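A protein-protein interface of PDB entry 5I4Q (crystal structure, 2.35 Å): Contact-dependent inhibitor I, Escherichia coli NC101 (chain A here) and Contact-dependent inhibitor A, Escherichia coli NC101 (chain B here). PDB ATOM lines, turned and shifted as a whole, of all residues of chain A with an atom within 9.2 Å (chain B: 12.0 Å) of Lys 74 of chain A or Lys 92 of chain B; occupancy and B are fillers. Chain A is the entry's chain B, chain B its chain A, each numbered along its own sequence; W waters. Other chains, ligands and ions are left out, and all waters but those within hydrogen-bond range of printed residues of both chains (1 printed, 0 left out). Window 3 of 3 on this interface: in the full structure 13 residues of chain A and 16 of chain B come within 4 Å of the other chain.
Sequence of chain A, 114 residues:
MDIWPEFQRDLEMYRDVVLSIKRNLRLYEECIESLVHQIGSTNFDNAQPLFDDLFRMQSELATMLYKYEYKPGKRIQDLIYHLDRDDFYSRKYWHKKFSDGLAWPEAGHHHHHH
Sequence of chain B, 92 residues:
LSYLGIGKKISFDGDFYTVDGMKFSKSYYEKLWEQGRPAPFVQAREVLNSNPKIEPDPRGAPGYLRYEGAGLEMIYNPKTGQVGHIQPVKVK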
ATOM      1  N   LEU A  25       4.694 -11.377  10.655  1.00  0.00           N
ATOM      2  CA  LEU A  25       3.795 -11.436   9.520  1.00  0.00           C
ATOM      3  C   LEU A  25       3.769 -12.828   8.860  1.00  0.00           C
ATOM      4  O   LEU A  25       2.694 -13.293   8.470  1.00  0.00           O
ATOM      5  CB  LEU A  25       4.101 -10.347   8.494  1.00  0.00           C
ATOM      6  CG  LEU A  25       3.615  -8.942   8.909  1.00  0.00           C
ATOM      7  CD1 LEU A  25       4.052  -7.920   7.917  1.00  0.00           C
ATOM      8  CD2 LEU A  25       2.119  -8.821   9.089  1.00  0.00           C
ATOM      9  N   GLU A  29       0.474 -15.170   8.481  1.00  0.00           N
ATOM     10  CA  GLU A  29       0.154 -15.704   7.169  1.00  0.00           C
ATOM     11  C   GLU A  29      -0.079 -17.208   7.225  1.00  0.00           C
ATOM     12  O   GLU A  29      -1.055 -17.704   6.692  1.00  0.00           O
ATOM     13  CB  GLU A  29       1.249 -15.354   6.145  1.00  0.00           C
ATOM     14  CG  GLU A  29       0.712 -14.908   4.793  1.00  0.00           C
ATOM     15  CD  GLU A  29       1.789 -14.643   3.748  1.00  0.00           C
ATOM     16  OE1 GLU A  29       2.129 -15.607   3.022  1.00  0.00           O
ATOM     17  OE2 GLU A  29       2.254 -13.484   3.635  1.00  0.00           O
ATOM     18  N   LYS A  71       3.043  -0.923   6.530  1.00  0.00           N
ATOM     19  CA  LYS A  71       2.428  -1.369   5.276  1.00  0.00           C
ATOM     20  C   LYS A  71       3.013  -2.754   4.928  1.00  0.00           C
ATOM     21  O   LYS A  71       4.193  -2.877   4.715  1.00  0.00           O
ATOM     22  CB  LYS A  71       2.702  -0.326   4.181  1.00  0.00           C
ATOM     23  CG  LYS A  71       2.003  -0.620   2.854  1.00  0.00           C
ATOM     24  CD  LYS A  71       2.401   0.369   1.744  1.00  0.00           C
ATOM     25  CE  LYS A  71       1.690   0.104   0.399  1.00  0.00           C
ATOM     26  NZ  LYS A  71       2.231  -1.052  -0.393  1.00  0.00           N
ATOM     27  N   PRO A  72       2.195  -3.826   4.950  1.00  0.00           N
ATOM     28  CA  PRO A  72       2.712  -5.168   4.711  1.00  0.00           C
ATOM     29  C   PRO A  72       2.759  -5.536   3.211  1.00  0.00           C
ATOM     30  O   PRO A  72       2.389  -4.727   2.386  1.00  0.00           O
ATOM     31  CB  PRO A  72       1.678  -6.036   5.455  1.00  0.00           C
ATOM     32  CG  PRO A  72       0.401  -5.334   5.178  1.00  0.00           C
ATOM     33  CD  PRO A  72       0.777  -3.867   5.284  1.00  0.00           C
ATOM     34  N   GLY A  73       3.178  -6.762   2.882  1.00  0.00           N
ATOM     35  CA  GLY A  73       3.124  -7.268   1.507  1.00  0.00           C
ATOM     36  C   GLY A  73       1.706  -7.340   0.957  1.00  0.00           C
ATOM     37  O   GLY A  73       0.775  -7.526   1.697  1.00  0.00           O
ATOM     38  N   LYS A  74       1.567  -7.209  -0.360  1.00  0.00           N
ATOM     39  CA  LYS A  74       0.281  -7.236  -1.082  1.00  0.00           C
ATOM     40  C   LYS A  74      -0.681  -8.317  -0.615  1.00  0.00           C
ATOM     41  O   LYS A  74      -1.866  -8.075  -0.486  1.00  0.00           O
ATOM     42  CB  LYS A  74       0.547  -7.414  -2.583  1.00  0.00           C
ATOM     43  CG  LYS A  74      -0.682  -7.389  -3.493  1.00  0.00           C
ATOM     44  CD  LYS A  74      -1.192  -5.978  -3.799  1.00  0.00           C
ATOM     45  CE  LYS A  74      -2.577  -5.996  -4.469  1.00  0.00           C
ATOM     46  NZ  LYS A  74      -2.593  -6.572  -5.847  1.00  0.00           N
ATOM     47  N   ARG A  75      -0.167  -9.501  -0.360  1.00  0.00           N
ATOM     48  CA  ARG A  75      -0.988 -10.586   0.107  1.00  0.00           C
ATOM     49  C   ARG A  75      -1.757 -10.281   1.382  1.00  0.00           C
ATOM     50  O   ARG A  75      -2.988 -10.486   1.454  1.00  0.00           O
ATOM     51  CB  ARG A  75      -0.140 -11.841   0.304  1.00  0.00           C
ATOM     52  CG  ARG A  75      -0.880 -13.101  -0.089  1.00  0.00           C
ATOM     53  CD  ARG A  75       0.052 -14.293  -0.181  1.00  0.00           C
ATOM     54  NE  ARG A  75      -0.750 -15.472  -0.489  1.00  0.00           N
ATOM     55  CZ  ARG A  75      -0.927 -16.522   0.305  1.00  0.00           C
ATOM     56  NH1 ARG A  75      -0.323 -16.603   1.486  1.00  0.00           N
ATOM     57  NH2 ARG A  75      -1.702 -17.517  -0.103  1.00  0.00           N
ATOM     58  N   ILE A  76      -1.013  -9.840   2.390  1.00  0.00           N
ATOM     59  CA  ILE A  76      -1.585  -9.412   3.661  1.00  0.00           C
ATOM     60  C   ILE A  76      -2.465  -8.143   3.485  1.00  0.00           C
ATOM     61  O   ILE A  76      -3.482  -8.052   4.105  1.00  0.00           O
ATOM     62  CB  ILE A  76      -0.470  -9.117   4.667  1.00  0.00           C
ATOM     63  CG1 ILE A  76       0.357 -10.377   4.942  1.00  0.00           C
ATOM     64  CG2 ILE A  76      -1.015  -8.517   5.956  1.00  0.00           C
ATOM     65  CD1 ILE A  76      -0.331 -11.334   5.896  1.00  0.00           C
ATOM     66  N   GLN A  77      -2.088  -7.192   2.645  1.00  0.00           N
ATOM     67  CA  GLN A  77      -2.956  -6.049   2.338  1.00  0.00           C
ATOM     68  C   GLN A  77      -4.300  -6.451   1.753  1.00  0.00           C
ATOM     69  O   GLN A  77      -5.324  -5.945   2.156  1.00  0.00           O
ATOM     70  CB  GLN A  77      -2.313  -5.079   1.381  1.00  0.00           C
ATOM     71  CG  GLN A  77      -1.839  -3.788   2.005  1.00  0.00           C
ATOM     72  CD  GLN A  77      -0.900  -3.021   1.071  1.00  0.00           C
ATOM     73  OE1 GLN A  77       0.247  -3.434   0.835  1.00  0.00           O
ATOM     74  NE2 GLN A  77      -1.376  -1.909   0.539  1.00  0.00           N
ATOM     75  N   ASP A  78      -4.292  -7.366   0.804  1.00  0.00           N
ATOM     76  CA  ASP A  78      -5.517  -7.902   0.246  1.00  0.00           C
ATOM     77  C   ASP A  78      -6.326  -8.620   1.281  1.00  0.00           C
ATOM     78  O   ASP A  78      -7.539  -8.422   1.349  1.00  0.00           O
ATOM     79  CB  ASP A  78      -5.236  -8.845  -0.917  1.00  0.00           C
ATOM     80  CG  ASP A  78      -4.717  -8.111  -2.144  1.00  0.00           C
ATOM     81  OD1 ASP A  78      -4.896  -6.860  -2.271  1.00  0.00           O
ATOM     82  OD2 ASP A  78      -4.108  -8.789  -2.989  1.00  0.00           O
ATOM     83  N   LEU A  79      -5.671  -9.401   2.116  1.00  0.00           N
ATOM     84  CA  LEU A  79      -6.361 -10.041   3.201  1.00  0.00           C
ATOM     85  C   LEU A  79      -7.037  -9.055   4.161  1.00  0.00           C
ATOM     86  O   LEU A  79      -8.194  -9.274   4.568  1.00  0.00           O
ATOM     87  CB  LEU A  79      -5.425 -10.924   4.013  1.00  0.00           C
ATOM     88  CG  LEU A  79      -6.235 -11.544   5.163  1.00  0.00           C
ATOM     89  CD1 LEU A  79      -6.047 -13.051   5.195  1.00  0.00           C
ATOM     90  CD2 LEU A  79      -5.999 -10.882   6.520  1.00  0.00           C
ATOM     91  N   ILE A  80      -6.320  -7.999   4.551  1.00  0.00           N
ATOM     92  CA  ILE A  80      -6.884  -6.984   5.445  1.00  0.00           C
ATOM     93  C   ILE A  80      -8.153  -6.339   4.855  1.00  0.00           C
ATOM     94  O   ILE A  80      -9.143  -6.116   5.555  1.00  0.00           O
ATOM     95  CB  ILE A  80      -5.875  -5.905   5.782  1.00  0.00           C
ATOM     96  CG1 ILE A  80      -4.750  -6.450   6.697  1.00  0.00           C
ATOM     97  CG2 ILE A  80      -6.560  -4.721   6.440  1.00  0.00           C
ATOM     98  CD1 ILE A  80      -3.666  -5.419   6.915  1.00  0.00           C
ATOM     99  N   TYR A  81      -8.134  -6.064   3.567  1.00  0.00           N
ATOM    100  CA  TYR A  81      -9.331  -5.553   2.900  1.00  0.00           C
ATOM    101  C   TYR A  81     -10.461  -6.598   2.861  1.00  0.00           C
ATOM    102  O   TYR A  81     -11.556  -6.419   3.405  1.00  0.00           O
ATOM    103  CB  TYR A  81      -8.972  -5.075   1.484  1.00  0.00           C
ATOM    104  CG  TYR A  81     -10.195  -4.769   0.687  1.00  0.00           C
ATOM    105  CD1 TYR A  81     -10.881  -3.541   0.842  1.00  0.00           C
ATOM    106  CD2 TYR A  81     -10.723  -5.711  -0.189  1.00  0.00           C
ATOM    107  CE1 TYR A  81     -12.052  -3.283   0.147  1.00  0.00           C
ATOM    108  CE2 TYR A  81     -11.884  -5.445  -0.896  1.00  0.00           C
ATOM    109  CZ  TYR A  81     -12.531  -4.236  -0.726  1.00  0.00           C
ATOM    110  OH  TYR A  81     -13.685  -4.024  -1.407  1.00  0.00           O
ATOM    111  N   HIS A  82     -10.219  -7.707   2.210  1.00  0.00           N
ATOM    112  CA  HIS A  82     -11.307  -8.701   2.003  1.00  0.00           C
ATOM    113  C   HIS A  82     -11.975  -9.236   3.266  1.00  0.00           C
ATOM    114  O   HIS A  82     -13.167  -9.522   3.244  1.00  0.00           O
ATOM    115  CB  HIS A  82     -10.786  -9.874   1.214  1.00  0.00           C
ATOM    116  CG  HIS A  82     -10.399  -9.524  -0.187  1.00  0.00           C
ATOM    117  ND1 HIS A  82     -11.328  -9.154  -1.136  1.00  0.00           N
ATOM    118  CD2 HIS A  82      -9.207  -9.568  -0.822  1.00  0.00           C
ATOM    119  CE1 HIS A  82     -10.712  -8.933  -2.282  1.00  0.00           C
ATOM    120  NE2 HIS A  82      -9.427  -9.187  -2.120  1.00  0.00           N
ATOM    121  N   TRP A 104      -7.050 -18.619   0.047  1.00  0.00           N
ATOM    122  CA  TRP A 104      -6.706 -17.294   0.552  1.00  0.00           C
ATOM    123  C   TRP A 104      -7.789 -16.326   0.062  1.00  0.00           C
ATOM    124  O   TRP A 104      -8.246 -16.449  -1.045  1.00  0.00           O
ATOM    125  CB  TRP A 104      -5.340 -16.883   0.006  1.00  0.00           C
ATOM    126  CG  TRP A 104      -4.776 -15.685   0.664  1.00  0.00           C
ATOM    127  CD1 TRP A 104      -4.783 -14.419   0.185  1.00  0.00           C
ATOM    128  CD2 TRP A 104      -4.121 -15.627   1.940  1.00  0.00           C
ATOM    129  NE1 TRP A 104      -4.189 -13.563   1.080  1.00  0.00           N
ATOM    130  CE2 TRP A 104      -3.766 -14.277   2.166  1.00  0.00           C
ATOM    131  CE3 TRP A 104      -3.799 -16.579   2.914  1.00  0.00           C
ATOM    132  CZ2 TRP A 104      -3.088 -13.857   3.321  1.00  0.00           C
ATOM    133  CZ3 TRP A 104      -3.144 -16.155   4.074  1.00  0.00           C
ATOM    134  CH2 TRP A 104      -2.781 -14.806   4.252  1.00  0.00           C
ATOM    135  N   PRO A 105      -8.199 -15.358   0.862  1.00  0.00           N
ATOM    136  CA  PRO A 105      -9.227 -14.423   0.389  1.00  0.00           C
ATOM    137  C   PRO A 105      -8.908 -13.628  -0.885  1.00  0.00           C
ATOM    138  O   PRO A 105      -7.808 -13.140  -1.070  1.00  0.00           O
ATOM    139  CB  PRO A 105      -9.382 -13.462   1.554  1.00  0.00           C
ATOM    140  CG  PRO A 105      -8.939 -14.224   2.727  1.00  0.00           C
ATOM    141  CD  PRO A 105      -7.863 -15.143   2.270  1.00  0.00           C
ATOM    142  N   ARG B  66     -24.472  -1.002  -0.552  1.00  0.00           N
ATOM    143  CA  ARG B  66     -23.093  -0.610  -0.629  1.00  0.00           C
ATOM    144  C   ARG B  66     -22.936   0.765  -1.274  1.00  0.00           C
ATOM    145  O   ARG B  66     -23.342   0.956  -2.403  1.00  0.00           O
ATOM    146  CB  ARG B  66     -22.346  -1.608  -1.435  1.00  0.00           C
ATOM    147  CG  ARG B  66     -20.841  -1.528  -1.301  1.00  0.00           C
ATOM    148  CD  ARG B  66     -20.234  -2.084  -2.577  1.00  0.00           C
ATOM    149  NE  ARG B  66     -18.773  -2.133  -2.520  1.00  0.00           N
ATOM    150  CZ  ARG B  66     -17.938  -1.356  -3.219  1.00  0.00           C
ATOM    151  NH1 ARG B  66     -18.389  -0.419  -4.063  1.00  0.00           N
ATOM    152  NH2 ARG B  66     -16.627  -1.510  -3.052  1.00  0.00           N
ATOM    153  N   GLU B  68     -20.016   3.780  -2.214  1.00  0.00           N
ATOM    154  CA  GLU B  68     -18.609   3.981  -2.455  1.00  0.00           C
ATOM    155  C   GLU B  68     -18.311   5.419  -2.855  1.00  0.00           C
ATOM    156  O   GLU B  68     -18.833   5.903  -3.842  1.00  0.00           O
ATOM    157  CB  GLU B  68     -18.126   3.056  -3.551  1.00  0.00           C
ATOM    158  CG  GLU B  68     -16.594   3.052  -3.678  1.00  0.00           C
ATOM    159  CD  GLU B  68     -16.064   1.948  -4.584  1.00  0.00           C
ATOM    160  OE1 GLU B  68     -16.894   1.148  -5.097  1.00  0.00           O
ATOM    161  OE2 GLU B  68     -14.831   1.889  -4.797  1.00  0.00           O
ATOM    162  N   GLY B  71     -13.024   7.787  -1.119  1.00  0.00           N
ATOM    163  CA  GLY B  71     -11.971   6.845  -0.754  1.00  0.00           C
ATOM    164  C   GLY B  71     -12.422   5.678   0.129  1.00  0.00           C
ATOM    165  O   GLY B  71     -11.619   4.926   0.587  1.00  0.00           O
ATOM    166  N   GLU B  73     -15.692   2.627   1.258  1.00  0.00           N
ATOM    167  CA  GLU B  73     -16.787   1.738   0.940  1.00  0.00           C
ATOM    168  C   GLU B  73     -17.482   1.542   2.237  1.00  0.00           C
ATOM    169  O   GLU B  73     -16.858   1.270   3.293  1.00  0.00           O
ATOM    170  CB  GLU B  73     -16.363   0.341   0.482  1.00  0.00           C
ATOM    171  CG  GLU B  73     -15.436   0.314  -0.724  1.00  0.00           C
ATOM    172  CD  GLU B  73     -14.748  -1.049  -0.973  1.00  0.00           C
ATOM    173  OE1 GLU B  73     -15.051  -2.017  -0.243  1.00  0.00           O
ATOM    174  OE2 GLU B  73     -13.886  -1.134  -1.910  1.00  0.00           O
ATOM    175  N   GLN B  87     -14.777   0.948   5.463  1.00  0.00           N
ATOM    176  CA  GLN B  87     -13.319   0.793   5.351  1.00  0.00           C
ATOM    177  C   GLN B  87     -12.814   1.497   4.082  1.00  0.00           C
ATOM    178  O   GLN B  87     -13.633   1.789   3.174  1.00  0.00           O
ATOM    179  CB  GLN B  87     -12.936  -0.677   5.311  1.00  0.00           C
ATOM    180  CG  GLN B  87     -13.179  -1.380   4.000  1.00  0.00           C
ATOM    181  CD  GLN B  87     -12.495  -2.765   3.928  1.00  0.00           C
ATOM    182  OE1 GLN B  87     -11.334  -2.959   4.336  1.00  0.00           O
ATOM    183  NE2 GLN B  87     -13.183  -3.685   3.362  1.00  0.00           N
ATOM    184  N   PRO B  88     -11.487   1.763   3.998  1.00  0.00           N
ATOM    185  CA  PRO B  88     -10.939   2.359   2.755  1.00  0.00           C
ATOM    186  C   PRO B  88     -11.085   1.420   1.571  1.00  0.00           C
ATOM    187  O   PRO B  88     -11.199   0.221   1.761  1.00  0.00           O
ATOM    188  CB  PRO B  88      -9.458   2.640   3.122  1.00  0.00           C
ATOM    189  CG  PRO B  88      -9.481   2.781   4.627  1.00  0.00           C
ATOM    190  CD  PRO B  88     -10.448   1.700   5.037  1.00  0.00           C
ATOM    191  N   VAL B  89     -11.160   1.928   0.363  1.00  0.00           N
ATOM    192  CA  VAL B  89     -11.292   1.019  -0.788  1.00  0.00           C
ATOM    193  C   VAL B  89     -10.041   0.183  -0.949  1.00  0.00           C
ATOM    194  O   VAL B  89      -8.983   0.546  -0.446  1.00  0.00           O
ATOM    195  CB  VAL B  89     -11.565   1.760  -2.108  1.00  0.00           C
ATOM    196  CG1 VAL B  89     -12.916   2.464  -2.044  1.00  0.00           C
ATOM    197  CG2 VAL B  89     -10.442   2.752  -2.456  1.00  0.00           C
ATOM    198  N   LYS B  90     -10.157  -0.909  -1.685  1.00  0.00           N
ATOM    199  CA  LYS B  90      -9.024  -1.754  -1.989  1.00  0.00           C
ATOM    200  C   LYS B  90      -7.940  -0.941  -2.686  1.00  0.00           C
ATOM    201  O   LYS B  90      -8.213  -0.155  -3.576  1.00  0.00           O
ATOM    202  CB  LYS B  90      -9.462  -2.953  -2.838  1.00  0.00           C
ATOM    203  CG  LYS B  90      -8.399  -4.032  -2.955  1.00  0.00           C
ATOM    204  CD  LYS B  90      -8.752  -5.056  -4.009  1.00  0.00           C
ATOM    205  CE  LYS B  90      -7.649  -6.081  -4.117  1.00  0.00           C
ATOM    206  NZ  LYS B  90      -8.062  -7.126  -5.079  1.00  0.00           N
ATOM    207  N   VAL B  91      -6.712  -1.090  -2.217  1.00  0.00           N
ATOM    208  CA  VAL B  91      -5.568  -0.475  -2.857  1.00  0.00           C
ATOM    209  C   VAL B  91      -5.199  -1.321  -4.077  1.00  0.00           C
ATOM    210  O   VAL B  91      -5.142  -2.553  -3.984  1.00  0.00           O
ATOM    211  CB  VAL B  91      -4.377  -0.398  -1.881  1.00  0.00           C
ATOM    212  CG1 VAL B  91      -3.106   0.024  -2.618  1.00  0.00           C
ATOM    213  CG2 VAL B  91      -4.689   0.561  -0.732  1.00  0.00           C
ATOM    214  N   LYS B  92      -4.965  -0.679  -5.220  1.00  0.00           N
ATOM    215  CA  LYS B  92      -4.427  -1.396  -6.382  1.00  0.00           C
ATOM    216  C   LYS B  92      -2.929  -1.679  -6.156  1.00  0.00           C
ATOM    217  O   LYS B  92      -2.401  -2.724  -6.531  1.00  0.00           O
ATOM    218  CB  LYS B  92      -4.651  -0.607  -7.674  1.00  0.00           C
ATOM    219  CG  LYS B  92      -4.327  -1.403  -8.938  1.00  0.00           C
ATOM    220  CD  LYS B  92      -4.086  -0.507 -10.154  1.00  0.00           C
ATOM    221  CE  LYS B  92      -3.164  -1.168 -11.173  1.00  0.00           C
ATOM    222  NZ  LYS B  92      -3.747  -2.404 -11.771  1.00  0.00           N
ATOM    223  OXT LYS B  92      -2.200  -0.874  -5.567  1.00  0.00           O
HETATM  224  O   HOH W   1     -14.377  -6.740   4.243  1.00  0.00           O
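The side-chain carboxylate of Glu 73 of chain B is in hydrogen-bond range of the side-chain hydroxyl of Tyr 81 of chain A (2.7 Å).
The side-chain amide nitrogen (NE2) of Gln 87 of chain B lies within hydrogen-bond range of the backbone carbonyl oxygen (O) of Tyr 81 of chain A (3.2 Å).
The chain-end carboxylate (O) of Lys 92 of chain B lies within salt-bridge range of the side-chain amino group (NZ) of Lys 74 of chain A.
OE2 of Glu 73 of chain B is in salt-bridge range of NH2 of Arg 66 of chain B, 3.0 Å away.
N of Glu 73 of chain B is in hydrogen-bond range of O of Gln 87 of chain B, at 2.9 Å.
NZ of Lys 74 of chain A is in salt-bridge range of OD2 of Asp 78 of chain A (3.9 Å).
Among the printed residues, pairs that only touch across the chains: Asp 78 of chain A with Lys 90 of chain B, Tyr 81 of chain A with Pro 88 of chain B, Tyr 81 of chain A with Lys 90 of chain B and His 82 of chain A with Lys 90 of chain B.
Lys 74 of chain A touches just one residue of chain B: Lys 92 (3.9 Å).
Of the printed residues of chain A, Lys 92 of chain B touches Lys 74 (3.9 Å).
No residue of chain B comes within 4 Å of Pro 72 of chain A.
No residue of chain B comes within 4 Å of Gly 73 of chain A.
No residue of chain B comes within 4 Å of Gln 77 of chain A.
Printed residues of chain B within 4 Å of Asp 78 of chain A: Lys 90.
No residue of chain A comes within 4 Å of Val 91 of chain B.
Printed residues of chain A within 4 Å of Lys 90 of chain B: Asp 78 (3.4 Å), Tyr 81 (3.5 Å) and His 82 (3.9 Å).
Of the printed residues of chain A, Gln 87 of chain B touches Tyr 81.
Trp 104 of chain A touches none of the printed residues of chain B.
Arg 75 of chain A touches none of the printed residues of chain B.
The nearest printed residue of chain A that does not touch Gln 87 of chain B is Ile 80 of chain A (4.03 Å).
Printed residues of chain A that touch a printed residue of chain B: Lys 74, Asp 78, Tyr 81 and His 82.
Hydrophobic or aromatic side chains of chain A within 4 Å of the printed part of chain B: Tyr 81 and His 82.
Printed residues of chain B that touch a printed residue of chain A: Glu 73, Gln 87, Pro 88, Lys 90 and Lys 92.
Among the printed residues, 7 pairs touch across the chains.
Water W1 lies within hydrogen-bond range of O of Tyr 81 of chain A, O of His 82 of chain A and NE2 of Gln 87 of chain B.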
